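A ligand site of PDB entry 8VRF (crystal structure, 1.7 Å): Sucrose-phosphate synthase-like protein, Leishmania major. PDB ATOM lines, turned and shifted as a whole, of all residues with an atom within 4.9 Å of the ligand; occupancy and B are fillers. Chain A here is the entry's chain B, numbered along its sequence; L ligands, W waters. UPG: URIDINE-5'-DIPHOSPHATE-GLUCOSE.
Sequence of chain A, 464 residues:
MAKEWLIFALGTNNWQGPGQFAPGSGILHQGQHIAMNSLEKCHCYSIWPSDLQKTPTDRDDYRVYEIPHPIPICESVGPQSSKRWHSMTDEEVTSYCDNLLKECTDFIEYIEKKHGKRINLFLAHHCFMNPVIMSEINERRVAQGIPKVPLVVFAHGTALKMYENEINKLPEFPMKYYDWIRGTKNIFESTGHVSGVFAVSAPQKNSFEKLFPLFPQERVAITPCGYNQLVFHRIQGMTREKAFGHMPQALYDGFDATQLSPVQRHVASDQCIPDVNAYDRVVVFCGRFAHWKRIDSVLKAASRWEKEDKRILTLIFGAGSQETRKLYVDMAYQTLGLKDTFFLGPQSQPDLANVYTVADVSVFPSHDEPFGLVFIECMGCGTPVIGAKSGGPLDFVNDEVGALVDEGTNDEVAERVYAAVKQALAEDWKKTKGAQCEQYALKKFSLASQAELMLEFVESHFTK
O1B of the ligand sits at hydrogen-bond distance from N of Gly 24, at 3.0 Å.
O2C of the ligand sits at hydrogen-bond distance from NE2 of Gln 349 (2.8 Å).
OE2 of Glu 369 lies within hydrogen-bond range of O3' of the ligand (2.5 Å).
The backbone NH (N) of Arg 288 sits at hydrogen-bond distance from an oxygen (O1A) of the ligand (2.8 Å).
The backbone NH of Gly 372 sits at hydrogen-bond distance from an oxygen (O3') of the ligand (2.9 Å).
O2B of the ligand is in salt-bridge range of NE of Arg 288.
NZ of Lys 293 lies within salt-bridge range of O2A of the ligand, at 2.8 Å.
The backbone carbonyl oxygen (O) of Gln 347 is in hydrogen-bond range of a nitrogen (N3) of the ligand (2.8 Å).
An oxygen (O4') of the ligand lies within hydrogen-bond range of the backbone NH (N) of Leu 373 (3.1 Å).
The backbone NH of Val 374 sits close to an oxygen (O3C) of the ligand.
The side-chain amide nitrogen (NE2) of Gln 16 is in hydrogen-bond range of an oxygen (O2) of the ligand, at 2.9 Å.
The side-chain carboxylate (OE2) of Glu 377 is in hydrogen-bond range of an oxygen (O2C) of the ligand, at 2.7 Å.
An oxygen (O3') of the ligand is in hydrogen-bond range of the backbone NH (N) of Phe 371, at 2.9 Å.
An oxygen (O4) of the ligand sits at hydrogen-bond distance from the backbone NH of Gln 347 (3.1 Å).
The backbone carbonyl oxygen (O) of Gly 345 lies within hydrogen-bond range of the backbone NH (N) of Gly 318 (3.0 Å).
N of Ala 22 lies within hydrogen-bond range of OE1 of Gln 16 (3.0 Å).
OE1 of Glu 369 lies within salt-bridge range of NZ of Lys 293.
The backbone carbonyl oxygen (O) of Phe 317 lies within hydrogen-bond range of the backbone NH (N) of Gly 287, at 3.1 Å.
CG1 of Ile 27 touches O4C of the ligand (3.6 Å).
Leu 28 touches the ligand (CD2 to O6', 3.6 Å).
SG of Cys 286 touches C5 of the ligand, at 3.6 Å.
CA of Gly 287 touches O1A of the ligand, 3.2 Å away.
Trp 292 touches the ligand.
Gly 318 touches the ligand (CA to O4, 3.9 Å).
Pro 346 touches the ligand.
Leu 352 touches the ligand (CD1 to N3, 3.4 Å).
CD of Pro 370 touches O2' of the ligand, 3.5 Å away.
Hydrophobic or aromatic side chains that line the ligand: Ile 27, Leu 28, Trp 292, Pro 346, Leu 352, Pro 370, Phe 371, Leu 373 and Val 374.
Of the 30 residues printed, 21 come within 4 Å of the ligand.
The nearest printed residue that does not touch the ligand is Ser 25 (4.2 Å).
Water W2 lies within hydrogen-bond range of an oxygen (O4C) of the ligand (2.7 Å), the backbone carbonyl oxygen of Ala 22 (2.8 Å) and the backbone NH of Gly 24 (3.5 Å).
Water W5 bridges O1B of the ligand (2.7 Å) and N of Gly 24 (3.4 Å).
Water W8 bridges O1A of the ligand and N of Arg 288.
Water W1 lies within hydrogen-bond range of O2A of the ligand (2.8 Å), OE2 of Glu 369 (2.9 Å), N of Leu 373 (3.1 Å) and N of Val 374 (3.3 Å).
Water W9 lies within hydrogen-bond range of O1B of the ligand (2.9 Å), N of Ser 25 (3.1 Å) and N of Gly 24 (3.2 Å).
Water W6 lies within hydrogen-bond range of OE1 of Gln 16, O of Ala 22 and N3 of the ligand.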
ATOM      1  N   GLN A  16     -19.855   7.330  -7.362  1.00  0.00           N
ATOM      2  CA  GLN A  16     -18.648   6.534  -7.208  1.00  0.00           C
ATOM      3  C   GLN A  16     -17.581   7.355  -6.493  1.00  0.00           C
ATOM      4  O   GLN A  16     -17.149   8.404  -6.950  1.00  0.00           O
ATOM      5  CB  GLN A  16     -18.149   6.121  -8.596  1.00  0.00           C
ATOM      6  CG  GLN A  16     -16.921   5.230  -8.544  1.00  0.00           C
ATOM      7  CD  GLN A  16     -17.022   4.159  -9.618  1.00  0.00           C
ATOM      8  OE1 GLN A  16     -17.913   3.314  -9.587  1.00  0.00           O
ATOM      9  NE2 GLN A  16     -16.113   4.162 -10.560  1.00  0.00           N
ATOM     10  N   PHE A  21     -18.273   1.836  -5.076  1.00  0.00           N
ATOM     11  CA  PHE A  21     -18.557   1.892  -6.505  1.00  0.00           C
ATOM     12  C   PHE A  21     -20.027   2.215  -6.684  1.00  0.00           C
ATOM     13  O   PHE A  21     -20.859   2.024  -5.778  1.00  0.00           O
ATOM     14  CB  PHE A  21     -18.179   0.574  -7.186  1.00  0.00           C
ATOM     15  CG  PHE A  21     -16.676   0.335  -7.203  1.00  0.00           C
ATOM     16  CD1 PHE A  21     -15.884   0.949  -8.157  1.00  0.00           C
ATOM     17  CD2 PHE A  21     -16.083  -0.502  -6.275  1.00  0.00           C
ATOM     18  CE1 PHE A  21     -14.510   0.774  -8.142  1.00  0.00           C
ATOM     19  CE2 PHE A  21     -14.715  -0.725  -6.306  1.00  0.00           C
ATOM     20  CZ  PHE A  21     -13.933  -0.052  -7.199  1.00  0.00           C
ATOM     21  N   ALA A  22     -20.350   2.746  -7.874  1.00  0.00           N
ATOM     22  CA  ALA A  22     -21.689   3.193  -8.187  1.00  0.00           C
ATOM     23  C   ALA A  22     -22.259   2.281  -9.272  1.00  0.00           C
ATOM     24  O   ALA A  22     -21.561   1.945 -10.214  1.00  0.00           O
ATOM     25  CB  ALA A  22     -21.660   4.616  -8.706  1.00  0.00           C
ATOM     26  N   PRO A  23     -23.582   2.030  -9.252  1.00  0.00           N
ATOM     27  CA  PRO A  23     -24.265   1.454 -10.408  1.00  0.00           C
ATOM     28  C   PRO A  23     -24.338   2.423 -11.578  1.00  0.00           C
ATOM     29  O   PRO A  23     -24.125   3.637 -11.431  1.00  0.00           O
ATOM     30  CB  PRO A  23     -25.668   1.140  -9.845  1.00  0.00           C
ATOM     31  CG  PRO A  23     -25.894   2.244  -8.844  1.00  0.00           C
ATOM     32  CD  PRO A  23     -24.500   2.466  -8.202  1.00  0.00           C
ATOM     33  N   GLY A  24     -24.674   1.901 -12.749  1.00  0.00           N
ATOM     34  CA  GLY A  24     -24.671   2.706 -13.946  1.00  0.00           C
ATOM     35  C   GLY A  24     -25.527   3.969 -13.820  1.00  0.00           C
ATOM     36  O   GLY A  24     -25.102   5.045 -14.237  1.00  0.00           O
ATOM     37  N   SER A  25     -26.660   3.893 -13.098  1.00  0.00           N
ATOM     38  CA  SER A  25     -27.542   5.061 -12.955  1.00  0.00           C
ATOM     39  C   SER A  25     -26.929   6.121 -12.011  1.00  0.00           C
ATOM     40  O   SER A  25     -27.109   7.327 -12.197  1.00  0.00           O
ATOM     41  CB  SER A  25     -28.937   4.628 -12.582  1.00  0.00           C
ATOM     42  OG  SER A  25     -28.983   3.876 -11.355  1.00  0.00           O
ATOM     43  N   ILE A  27     -23.538   6.522 -11.887  1.00  0.00           N
ATOM     44  CA  ILE A  27     -22.512   7.049 -12.777  1.00  0.00           C
ATOM     45  C   ILE A  27     -23.132   8.124 -13.678  1.00  0.00           C
ATOM     46  O   ILE A  27     -22.518   9.165 -13.907  1.00  0.00           O
ATOM     47  CB  ILE A  27     -21.842   5.934 -13.596  1.00  0.00           C
ATOM     48  CG1 ILE A  27     -21.112   4.882 -12.740  1.00  0.00           C
ATOM     49  CG2 ILE A  27     -20.934   6.476 -14.703  1.00  0.00           C
ATOM     50  CD1 ILE A  27     -19.803   5.326 -12.083  1.00  0.00           C
ATOM     51  N   LEU A  28     -24.337   7.846 -14.173  1.00  0.00           N
ATOM     52  CA  LEU A  28     -24.985   8.755 -15.102  1.00  0.00           C
ATOM     53  C   LEU A  28     -25.323  10.059 -14.380  1.00  0.00           C
ATOM     54  O   LEU A  28     -25.092  11.146 -14.907  1.00  0.00           O
ATOM     55  CB  LEU A  28     -26.213   8.095 -15.742  1.00  0.00           C
ATOM     56  CG  LEU A  28     -26.762   8.862 -16.950  1.00  0.00           C
ATOM     57  CD1 LEU A  28     -25.779   8.720 -18.100  1.00  0.00           C
ATOM     58  CD2 LEU A  28     -28.083   8.306 -17.373  1.00  0.00           C
ATOM     59  N   VAL A 200     -33.507   6.236 -20.841  1.00  0.00           N
ATOM     60  CA  VAL A 200     -32.194   5.857 -21.344  1.00  0.00           C
ATOM     61  C   VAL A 200     -32.322   5.108 -22.671  1.00  0.00           C
ATOM     62  O   VAL A 200     -31.484   5.274 -23.544  1.00  0.00           O
ATOM     63  CB  VAL A 200     -31.335   5.077 -20.322  1.00  0.00           C
ATOM     64  CG1 VAL A 200     -30.072   4.502 -20.938  1.00  0.00           C
ATOM     65  CG2 VAL A 200     -30.975   5.989 -19.164  1.00  0.00           C
ATOM     66  N   PHE A 232     -11.718   9.599 -19.601  1.00  0.00           N
ATOM     67  CA  PHE A 232     -11.519   8.634 -20.670  1.00  0.00           C
ATOM     68  C   PHE A 232     -11.039   9.263 -21.973  1.00  0.00           C
ATOM     69  O   PHE A 232     -11.813   9.582 -22.872  1.00  0.00           O
ATOM     70  CB  PHE A 232     -12.798   7.856 -20.949  1.00  0.00           C
ATOM     71  CG  PHE A 232     -13.218   6.978 -19.788  1.00  0.00           C
ATOM     72  CD1 PHE A 232     -12.649   5.716 -19.588  1.00  0.00           C
ATOM     73  CD2 PHE A 232     -14.213   7.379 -18.910  1.00  0.00           C
ATOM     74  CE1 PHE A 232     -13.092   4.900 -18.572  1.00  0.00           C
ATOM     75  CE2 PHE A 232     -14.640   6.563 -17.889  1.00  0.00           C
ATOM     76  CZ  PHE A 232     -14.083   5.320 -17.718  1.00  0.00           C
ATOM     77  N   CYS A 286     -15.493  -5.084 -19.526  1.00  0.00           N
ATOM     78  CA  CYS A 286     -15.908  -4.367 -18.307  1.00  0.00           C
ATOM     79  C   CYS A 286     -17.430  -4.361 -18.220  1.00  0.00           C
ATOM     80  O   CYS A 286     -18.095  -3.980 -19.189  1.00  0.00           O
ATOM     81  CB  CYS A 286     -15.435  -2.926 -18.374  1.00  0.00           C
ATOM     82  SG  CYS A 286     -15.761  -1.958 -16.859  1.00  0.00           S
ATOM     83  N   GLY A 287     -17.970  -4.720 -17.051  1.00  0.00           N
ATOM     84  CA  GLY A 287     -19.394  -4.676 -16.797  1.00  0.00           C
ATOM     85  C   GLY A 287     -19.741  -5.371 -15.486  1.00  0.00           C
ATOM     86  O   GLY A 287     -19.024  -6.255 -15.062  1.00  0.00           O
ATOM     87  N   ARG A 288     -20.854  -4.974 -14.867  1.00  0.00           N
ATOM     88  CA  ARG A 288     -21.380  -5.770 -13.786  1.00  0.00           C
ATOM     89  C   ARG A 288     -21.716  -7.196 -14.244  1.00  0.00           C
ATOM     90  O   ARG A 288     -22.001  -7.458 -15.412  1.00  0.00           O
ATOM     91  CB  ARG A 288     -22.588  -5.037 -13.223  1.00  0.00           C
ATOM     92  CG  ARG A 288     -23.733  -4.913 -14.213  1.00  0.00           C
ATOM     93  CD  ARG A 288     -24.911  -4.444 -13.444  1.00  0.00           C
ATOM     94  NE  ARG A 288     -26.028  -4.069 -14.299  1.00  0.00           N
ATOM     95  CZ  ARG A 288     -27.275  -3.977 -13.893  1.00  0.00           C
ATOM     96  NH1 ARG A 288     -27.630  -4.405 -12.689  1.00  0.00           N
ATOM     97  NH2 ARG A 288     -28.159  -3.403 -14.700  1.00  0.00           N
ATOM     98  N   TRP A 292     -27.276 -10.856 -18.496  1.00  0.00           N
ATOM     99  CA  TRP A 292     -27.514 -10.320 -19.837  1.00  0.00           C
ATOM    100  C   TRP A 292     -26.245  -9.704 -20.421  1.00  0.00           C
ATOM    101  O   TRP A 292     -26.189  -9.468 -21.623  1.00  0.00           O
ATOM    102  CB  TRP A 292     -28.672  -9.315 -19.890  1.00  0.00           C
ATOM    103  CG  TRP A 292     -28.532  -8.178 -18.928  1.00  0.00           C
ATOM    104  CD1 TRP A 292     -28.975  -8.109 -17.640  1.00  0.00           C
ATOM    105  CD2 TRP A 292     -27.893  -6.902 -19.207  1.00  0.00           C
ATOM    106  NE1 TRP A 292     -28.644  -6.907 -17.097  1.00  0.00           N
ATOM    107  CE2 TRP A 292     -27.971  -6.146 -18.029  1.00  0.00           C
ATOM    108  CE3 TRP A 292     -27.217  -6.379 -20.307  1.00  0.00           C
ATOM    109  CZ2 TRP A 292     -27.436  -4.866 -17.942  1.00  0.00           C
ATOM    110  CZ3 TRP A 292     -26.715  -5.096 -20.231  1.00  0.00           C
ATOM    111  CH2 TRP A 292     -26.799  -4.369 -19.059  1.00  0.00           C
ATOM    112  N   LYS A 293     -25.216  -9.456 -19.609  1.00  0.00           N
ATOM    113  CA  LYS A 293     -23.953  -8.976 -20.136  1.00  0.00           C
ATOM    114  C   LYS A 293     -23.172 -10.041 -20.908  1.00  0.00           C
ATOM    115  O   LYS A 293     -22.244  -9.690 -21.647  1.00  0.00           O
ATOM    116  CB  LYS A 293     -23.145  -8.412 -18.952  1.00  0.00           C
ATOM    117  CG  LYS A 293     -23.549  -7.082 -18.423  1.00  0.00           C
ATOM    118  CD  LYS A 293     -23.153  -5.940 -19.350  1.00  0.00           C
ATOM    119  CE  LYS A 293     -23.253  -4.668 -18.581  1.00  0.00           C
ATOM    120  NZ  LYS A 293     -22.915  -3.535 -19.469  1.00  0.00           N
ATOM    121  N   PHE A 317     -13.109  -7.005 -15.971  1.00  0.00           N
ATOM    122  CA  PHE A 317     -13.418  -5.999 -14.967  1.00  0.00           C
ATOM    123  C   PHE A 317     -14.900  -5.981 -14.642  1.00  0.00           C
ATOM    124  O   PHE A 317     -15.761  -6.174 -15.519  1.00  0.00           O
ATOM    125  CB  PHE A 317     -13.048  -4.617 -15.469  1.00  0.00           C
ATOM    126  CG  PHE A 317     -11.575  -4.502 -15.721  1.00  0.00           C
ATOM    127  CD1 PHE A 317     -10.698  -4.281 -14.672  1.00  0.00           C
ATOM    128  CD2 PHE A 317     -11.045  -4.709 -16.991  1.00  0.00           C
ATOM    129  CE1 PHE A 317      -9.344  -4.219 -14.894  1.00  0.00           C
ATOM    130  CE2 PHE A 317      -9.687  -4.581 -17.209  1.00  0.00           C
ATOM    131  CZ  PHE A 317      -8.833  -4.342 -16.145  1.00  0.00           C
ATOM    132  N   GLY A 318     -15.188  -5.621 -13.395  1.00  0.00           N
ATOM    133  CA  GLY A 318     -16.529  -5.358 -12.925  1.00  0.00           C
ATOM    134  C   GLY A 318     -16.826  -6.160 -11.662  1.00  0.00           C
ATOM    135  O   GLY A 318     -16.086  -7.073 -11.273  1.00  0.00           O
ATOM    136  N   GLY A 345     -11.788  -7.398 -10.806  1.00  0.00           N
ATOM    137  CA  GLY A 345     -12.841  -6.791 -10.015  1.00  0.00           C
ATOM    138  C   GLY A 345     -13.240  -5.416 -10.549  1.00  0.00           C
ATOM    139  O   GLY A 345     -12.838  -5.006 -11.629  1.00  0.00           O
ATOM    140  N   PRO A 346     -14.051  -4.644  -9.792  1.00  0.00           N
ATOM    141  CA  PRO A 346     -14.425  -3.300 -10.216  1.00  0.00           C
ATOM    142  C   PRO A 346     -13.192  -2.416 -10.059  1.00  0.00           C
ATOM    143  O   PRO A 346     -12.358  -2.675  -9.194  1.00  0.00           O
ATOM    144  CB  PRO A 346     -15.539  -2.931  -9.268  1.00  0.00           C
ATOM    145  CG  PRO A 346     -15.204  -3.685  -8.009  1.00  0.00           C
ATOM    146  CD  PRO A 346     -14.619  -5.015  -8.477  1.00  0.00           C
ATOM    147  N   GLN A 347     -13.122  -1.385 -10.889  1.00  0.00           N
ATOM    148  CA  GLN A 347     -12.032  -0.421 -10.917  1.00  0.00           C
ATOM    149  C   GLN A 347     -12.592   0.987 -11.144  1.00  0.00           C
ATOM    150  O   GLN A 347     -13.650   1.178 -11.758  1.00  0.00           O
ATOM    151  CB  GLN A 347     -10.948  -0.726 -11.956  1.00  0.00           C
ATOM    152  CG  GLN A 347     -10.297  -2.101 -11.770  1.00  0.00           C
ATOM    153  CD  GLN A 347      -9.407  -2.177 -10.551  1.00  0.00           C
ATOM    154  OE1 GLN A 347      -8.829  -1.176 -10.147  1.00  0.00           O
ATOM    155  NE2 GLN A 347      -9.222  -3.373 -10.012  1.00  0.00           N
ATOM    156  N   SER A 348     -11.834   1.966 -10.614  1.00  0.00           N
ATOM    157  CA  SER A 348     -12.104   3.379 -10.792  1.00  0.00           C
ATOM    158  C   SER A 348     -12.146   3.728 -12.279  1.00  0.00           C
ATOM    159  O   SER A 348     -11.517   3.056 -13.106  1.00  0.00           O
ATOM    160  CB  SER A 348     -11.060   4.205 -10.060  1.00  0.00           C
ATOM    161  OG  SER A 348      -9.895   4.338 -10.860  1.00  0.00           O
ATOM    162  N   GLN A 349     -12.872   4.782 -12.622  1.00  0.00           N
ATOM    163  CA  GLN A 349     -12.876   5.232 -14.005  1.00  0.00           C
ATOM    164  C   GLN A 349     -11.458   5.597 -14.493  1.00  0.00           C
ATOM    165  O   GLN A 349     -11.081   5.223 -15.598  1.00  0.00           O
ATOM    166  CB  GLN A 349     -13.915   6.350 -14.177  1.00  0.00           C
ATOM    167  CG  GLN A 349     -15.368   5.892 -14.046  1.00  0.00           C
ATOM    168  CD  GLN A 349     -16.306   7.040 -14.377  1.00  0.00           C
ATOM    169  OE1 GLN A 349     -16.017   8.215 -14.071  1.00  0.00           O
ATOM    170  NE2 GLN A 349     -17.470   6.753 -14.956  1.00  0.00           N
ATOM    171  N   LEU A 352      -9.671   2.433 -15.369  1.00  0.00           N
ATOM    172  CA  LEU A 352     -10.175   1.846 -16.599  1.00  0.00           C
ATOM    173  C   LEU A 352      -9.658   2.594 -17.839  1.00  0.00           C
ATOM    174  O   LEU A 352      -9.327   1.964 -18.853  1.00  0.00           O
ATOM    175  CB  LEU A 352     -11.696   1.819 -16.540  1.00  0.00           C
ATOM    176  CG  LEU A 352     -12.302   0.784 -15.602  1.00  0.00           C
ATOM    177  CD1 LEU A 352     -13.769   1.027 -15.407  1.00  0.00           C
ATOM    178  CD2 LEU A 352     -12.014  -0.620 -16.101  1.00  0.00           C
ATOM    179  N   GLU A 369     -28.174  -4.246 -24.465  1.00  0.00           N
ATOM    180  CA  GLU A 369     -27.541  -3.233 -23.639  1.00  0.00           C
ATOM    181  C   GLU A 369     -28.389  -1.974 -23.745  1.00  0.00           C
ATOM    182  O   GLU A 369     -28.693  -1.550 -24.857  1.00  0.00           O
ATOM    183  CB  GLU A 369     -26.105  -3.002 -24.141  1.00  0.00           C
ATOM    184  CG  GLU A 369     -25.356  -1.850 -23.457  1.00  0.00           C
ATOM    185  CD  GLU A 369     -24.682  -2.194 -22.138  1.00  0.00           C
ATOM    186  OE1 GLU A 369     -24.338  -3.350 -21.901  1.00  0.00           O
ATOM    187  OE2 GLU A 369     -24.593  -1.246 -21.352  1.00  0.00           O
ATOM    188  N   PRO A 370     -28.859  -1.357 -22.636  1.00  0.00           N
ATOM    189  CA  PRO A 370     -29.713  -0.166 -22.723  1.00  0.00           C
ATOM    190  C   PRO A 370     -29.094   0.963 -23.538  1.00  0.00           C
ATOM    191  O   PRO A 370     -29.680   1.403 -24.526  1.00  0.00           O
ATOM    192  CB  PRO A 370     -29.893   0.192 -21.226  1.00  0.00           C
ATOM    193  CG  PRO A 370     -29.867  -1.160 -20.551  1.00  0.00           C
ATOM    194  CD  PRO A 370     -28.711  -1.840 -21.251  1.00  0.00           C
ATOM    195  N   PHE A 371     -27.882   1.413 -23.198  1.00  0.00           N
ATOM    196  CA  PHE A 371     -27.163   2.411 -23.978  1.00  0.00           C
ATOM    197  C   PHE A 371     -25.792   1.834 -24.343  1.00  0.00           C
ATOM    198  O   PHE A 371     -25.527   1.523 -25.514  1.00  0.00           O
ATOM    199  CB  PHE A 371     -27.087   3.798 -23.314  1.00  0.00           C
ATOM    200  CG  PHE A 371     -26.178   4.749 -24.104  1.00  0.00           C
ATOM    201  CD1 PHE A 371     -26.549   5.204 -25.367  1.00  0.00           C
ATOM    202  CD2 PHE A 371     -24.957   5.171 -23.586  1.00  0.00           C
ATOM    203  CE1 PHE A 371     -25.697   6.010 -26.115  1.00  0.00           C
ATOM    204  CE2 PHE A 371     -24.128   6.005 -24.299  1.00  0.00           C
ATOM    205  CZ  PHE A 371     -24.489   6.421 -25.582  1.00  0.00           C
ATOM    206  N   GLY A 372     -24.955   1.642 -23.297  1.00  0.00           N
ATOM    207  CA  GLY A 372     -23.615   1.101 -23.426  1.00  0.00           C
ATOM    208  C   GLY A 372     -22.535   2.160 -23.177  1.00  0.00           C
ATOM    209  O   GLY A 372     -21.635   2.316 -24.005  1.00  0.00           O
ATOM    210  N   LEU A 373     -22.521   2.782 -21.993  1.00  0.00           N
ATOM    211  CA  LEU A 373     -21.475   3.747 -21.673  1.00  0.00           C
ATOM    212  C   LEU A 373     -20.076   3.142 -21.845  1.00  0.00           C
ATOM    213  O   LEU A 373     -19.122   3.827 -22.214  1.00  0.00           O
ATOM    214  CB  LEU A 373     -21.709   4.184 -20.229  1.00  0.00           C
ATOM    215  CG  LEU A 373     -20.805   5.294 -19.712  1.00  0.00           C
ATOM    216  CD1 LEU A 373     -20.743   6.523 -20.580  1.00  0.00           C
ATOM    217  CD2 LEU A 373     -21.290   5.732 -18.341  1.00  0.00           C
ATOM    218  N   VAL A 374     -19.924   1.846 -21.496  1.00  0.00           N
ATOM    219  CA  VAL A 374     -18.631   1.176 -21.556  1.00  0.00           C
ATOM    220  C   VAL A 374     -18.018   1.293 -22.955  1.00  0.00           C
ATOM    221  O   VAL A 374     -16.797   1.512 -23.110  1.00  0.00           O
ATOM    222  CB  VAL A 374     -18.622  -0.287 -21.086  1.00  0.00           C
ATOM    223  CG1 VAL A 374     -18.827  -0.421 -19.577  1.00  0.00           C
ATOM    224  CG2 VAL A 374     -19.637  -1.141 -21.835  1.00  0.00           C
ATOM    225  N   GLU A 377     -16.840   5.037 -23.512  1.00  0.00           N
ATOM    226  CA  GLU A 377     -15.621   5.242 -22.742  1.00  0.00           C
ATOM    227  C   GLU A 377     -14.386   4.628 -23.409  1.00  0.00           C
ATOM    228  O   GLU A 377     -13.308   5.239 -23.453  1.00  0.00           O
ATOM    229  CB  GLU A 377     -15.859   4.665 -21.350  1.00  0.00           C
ATOM    230  CG  GLU A 377     -16.841   5.504 -20.527  1.00  0.00           C
ATOM    231  CD  GLU A 377     -17.263   4.881 -19.232  1.00  0.00           C
ATOM    232  OE1 GLU A 377     -17.082   3.632 -19.096  1.00  0.00           O
ATOM    233  OE2 GLU A 377     -17.779   5.640 -18.343  1.00  0.00           O
HETATM  234  N1  UPG L   1     -17.901   1.342 -14.099  1.00  0.00           N
HETATM  235  C2  UPG L   1     -16.791   1.667 -13.340  1.00  0.00           C
HETATM  236  N3  UPG L   1     -16.088   0.585 -12.903  1.00  0.00           N
HETATM  237  C4  UPG L   1     -16.352  -0.756 -13.128  1.00  0.00           C
HETATM  238  C5  UPG L   1     -17.521  -0.997 -13.909  1.00  0.00           C
HETATM  239  C6  UPG L   1     -18.242   0.036 -14.357  1.00  0.00           C
HETATM  240  O2  UPG L   1     -16.490   2.833 -13.089  1.00  0.00           O
HETATM  241  O4  UPG L   1     -15.606  -1.621 -12.693  1.00  0.00           O
HETATM  242  C1C UPG L   1     -18.683   2.472 -14.580  1.00  0.00           C
HETATM  243  C2C UPG L   1     -18.224   2.935 -15.965  1.00  0.00           C
HETATM  244  O2C UPG L   1     -18.391   4.332 -16.109  1.00  0.00           O
HETATM  245  C3C UPG L   1     -19.190   2.145 -16.839  1.00  0.00           C
HETATM  246  C4C UPG L   1     -20.471   2.287 -16.030  1.00  0.00           C
HETATM  247  O4C UPG L   1     -20.041   2.096 -14.663  1.00  0.00           O
HETATM  248  O3C UPG L   1     -19.386   2.658 -18.149  1.00  0.00           O
HETATM  249  C5C UPG L   1     -21.569   1.335 -16.357  1.00  0.00           C
HETATM  250  O5C UPG L   1     -21.110   0.004 -16.243  1.00  0.00           O
HETATM  251  PA  UPG L   1     -22.150  -1.206 -16.448  1.00  0.00           P
HETATM  252  O1A UPG L   1     -21.526  -2.434 -15.890  1.00  0.00           O
HETATM  253  O2A UPG L   1     -22.626  -1.203 -17.867  1.00  0.00           O
HETATM  254  O3A UPG L   1     -23.427  -0.833 -15.578  1.00  0.00           O
HETATM  255  PB  UPG L   1     -24.996  -0.818 -15.740  1.00  0.00           P
HETATM  256  O1B UPG L   1     -25.511  -0.474 -14.393  1.00  0.00           O
HETATM  257  O2B UPG L   1     -25.435  -2.115 -16.346  1.00  0.00           O
HETATM  258  O3B UPG L   1     -25.188   0.384 -16.780  1.00  0.00           O
HETATM  259  C1' UPG L   1     -26.475   0.875 -17.040  1.00  0.00           C
HETATM  260  C2' UPG L   1     -26.878   0.368 -18.433  1.00  0.00           C
HETATM  261  C3' UPG L   1     -25.975   1.002 -19.506  1.00  0.00           C
HETATM  262  C4' UPG L   1     -26.007   2.509 -19.344  1.00  0.00           C
HETATM  263  C5' UPG L   1     -25.594   2.908 -17.934  1.00  0.00           C
HETATM  264  C6' UPG L   1     -25.684   4.386 -17.669  1.00  0.00           C
HETATM  265  O2' UPG L   1     -26.830  -1.044 -18.461  1.00  0.00           O
HETATM  266  O3' UPG L   1     -26.269   0.585 -20.877  1.00  0.00           O
HETATM  267  O4' UPG L   1     -25.023   3.029 -20.221  1.00  0.00           O
HETATM  268  O5' UPG L   1     -26.444   2.289 -16.972  1.00  0.00           O
HETATM  269  O6' UPG L   1     -26.962   4.919 -17.924  1.00  0.00           O
HETATM  270  O   HOH W   1     -22.510   0.312 -20.161  1.00  0.00           O
HETATM  271  O   HOH W   2     -21.387   0.831 -12.759  1.00  0.00           O
HETATM  272  O   HOH W   3     -28.966  -1.908 -17.009  1.00  0.00           O
HETATM  273  O   HOH W   4     -29.085   4.112 -16.460  1.00  0.00           O
HETATM  274  O   HOH W   5     -24.378  -1.402 -12.160  1.00  0.00           O
HETATM  275  O   HOH W   6     -18.779   1.211 -10.996  1.00  0.00           O
HETATM  276  O   HOH W   7     -26.276   5.724 -20.468  1.00  0.00           O
HETATM  277  O   HOH W   8     -21.232  -1.916 -13.208  1.00  0.00           O
HETATM  278  O   HOH W   9     -27.743   0.948 -13.148  1.00  0.00           O
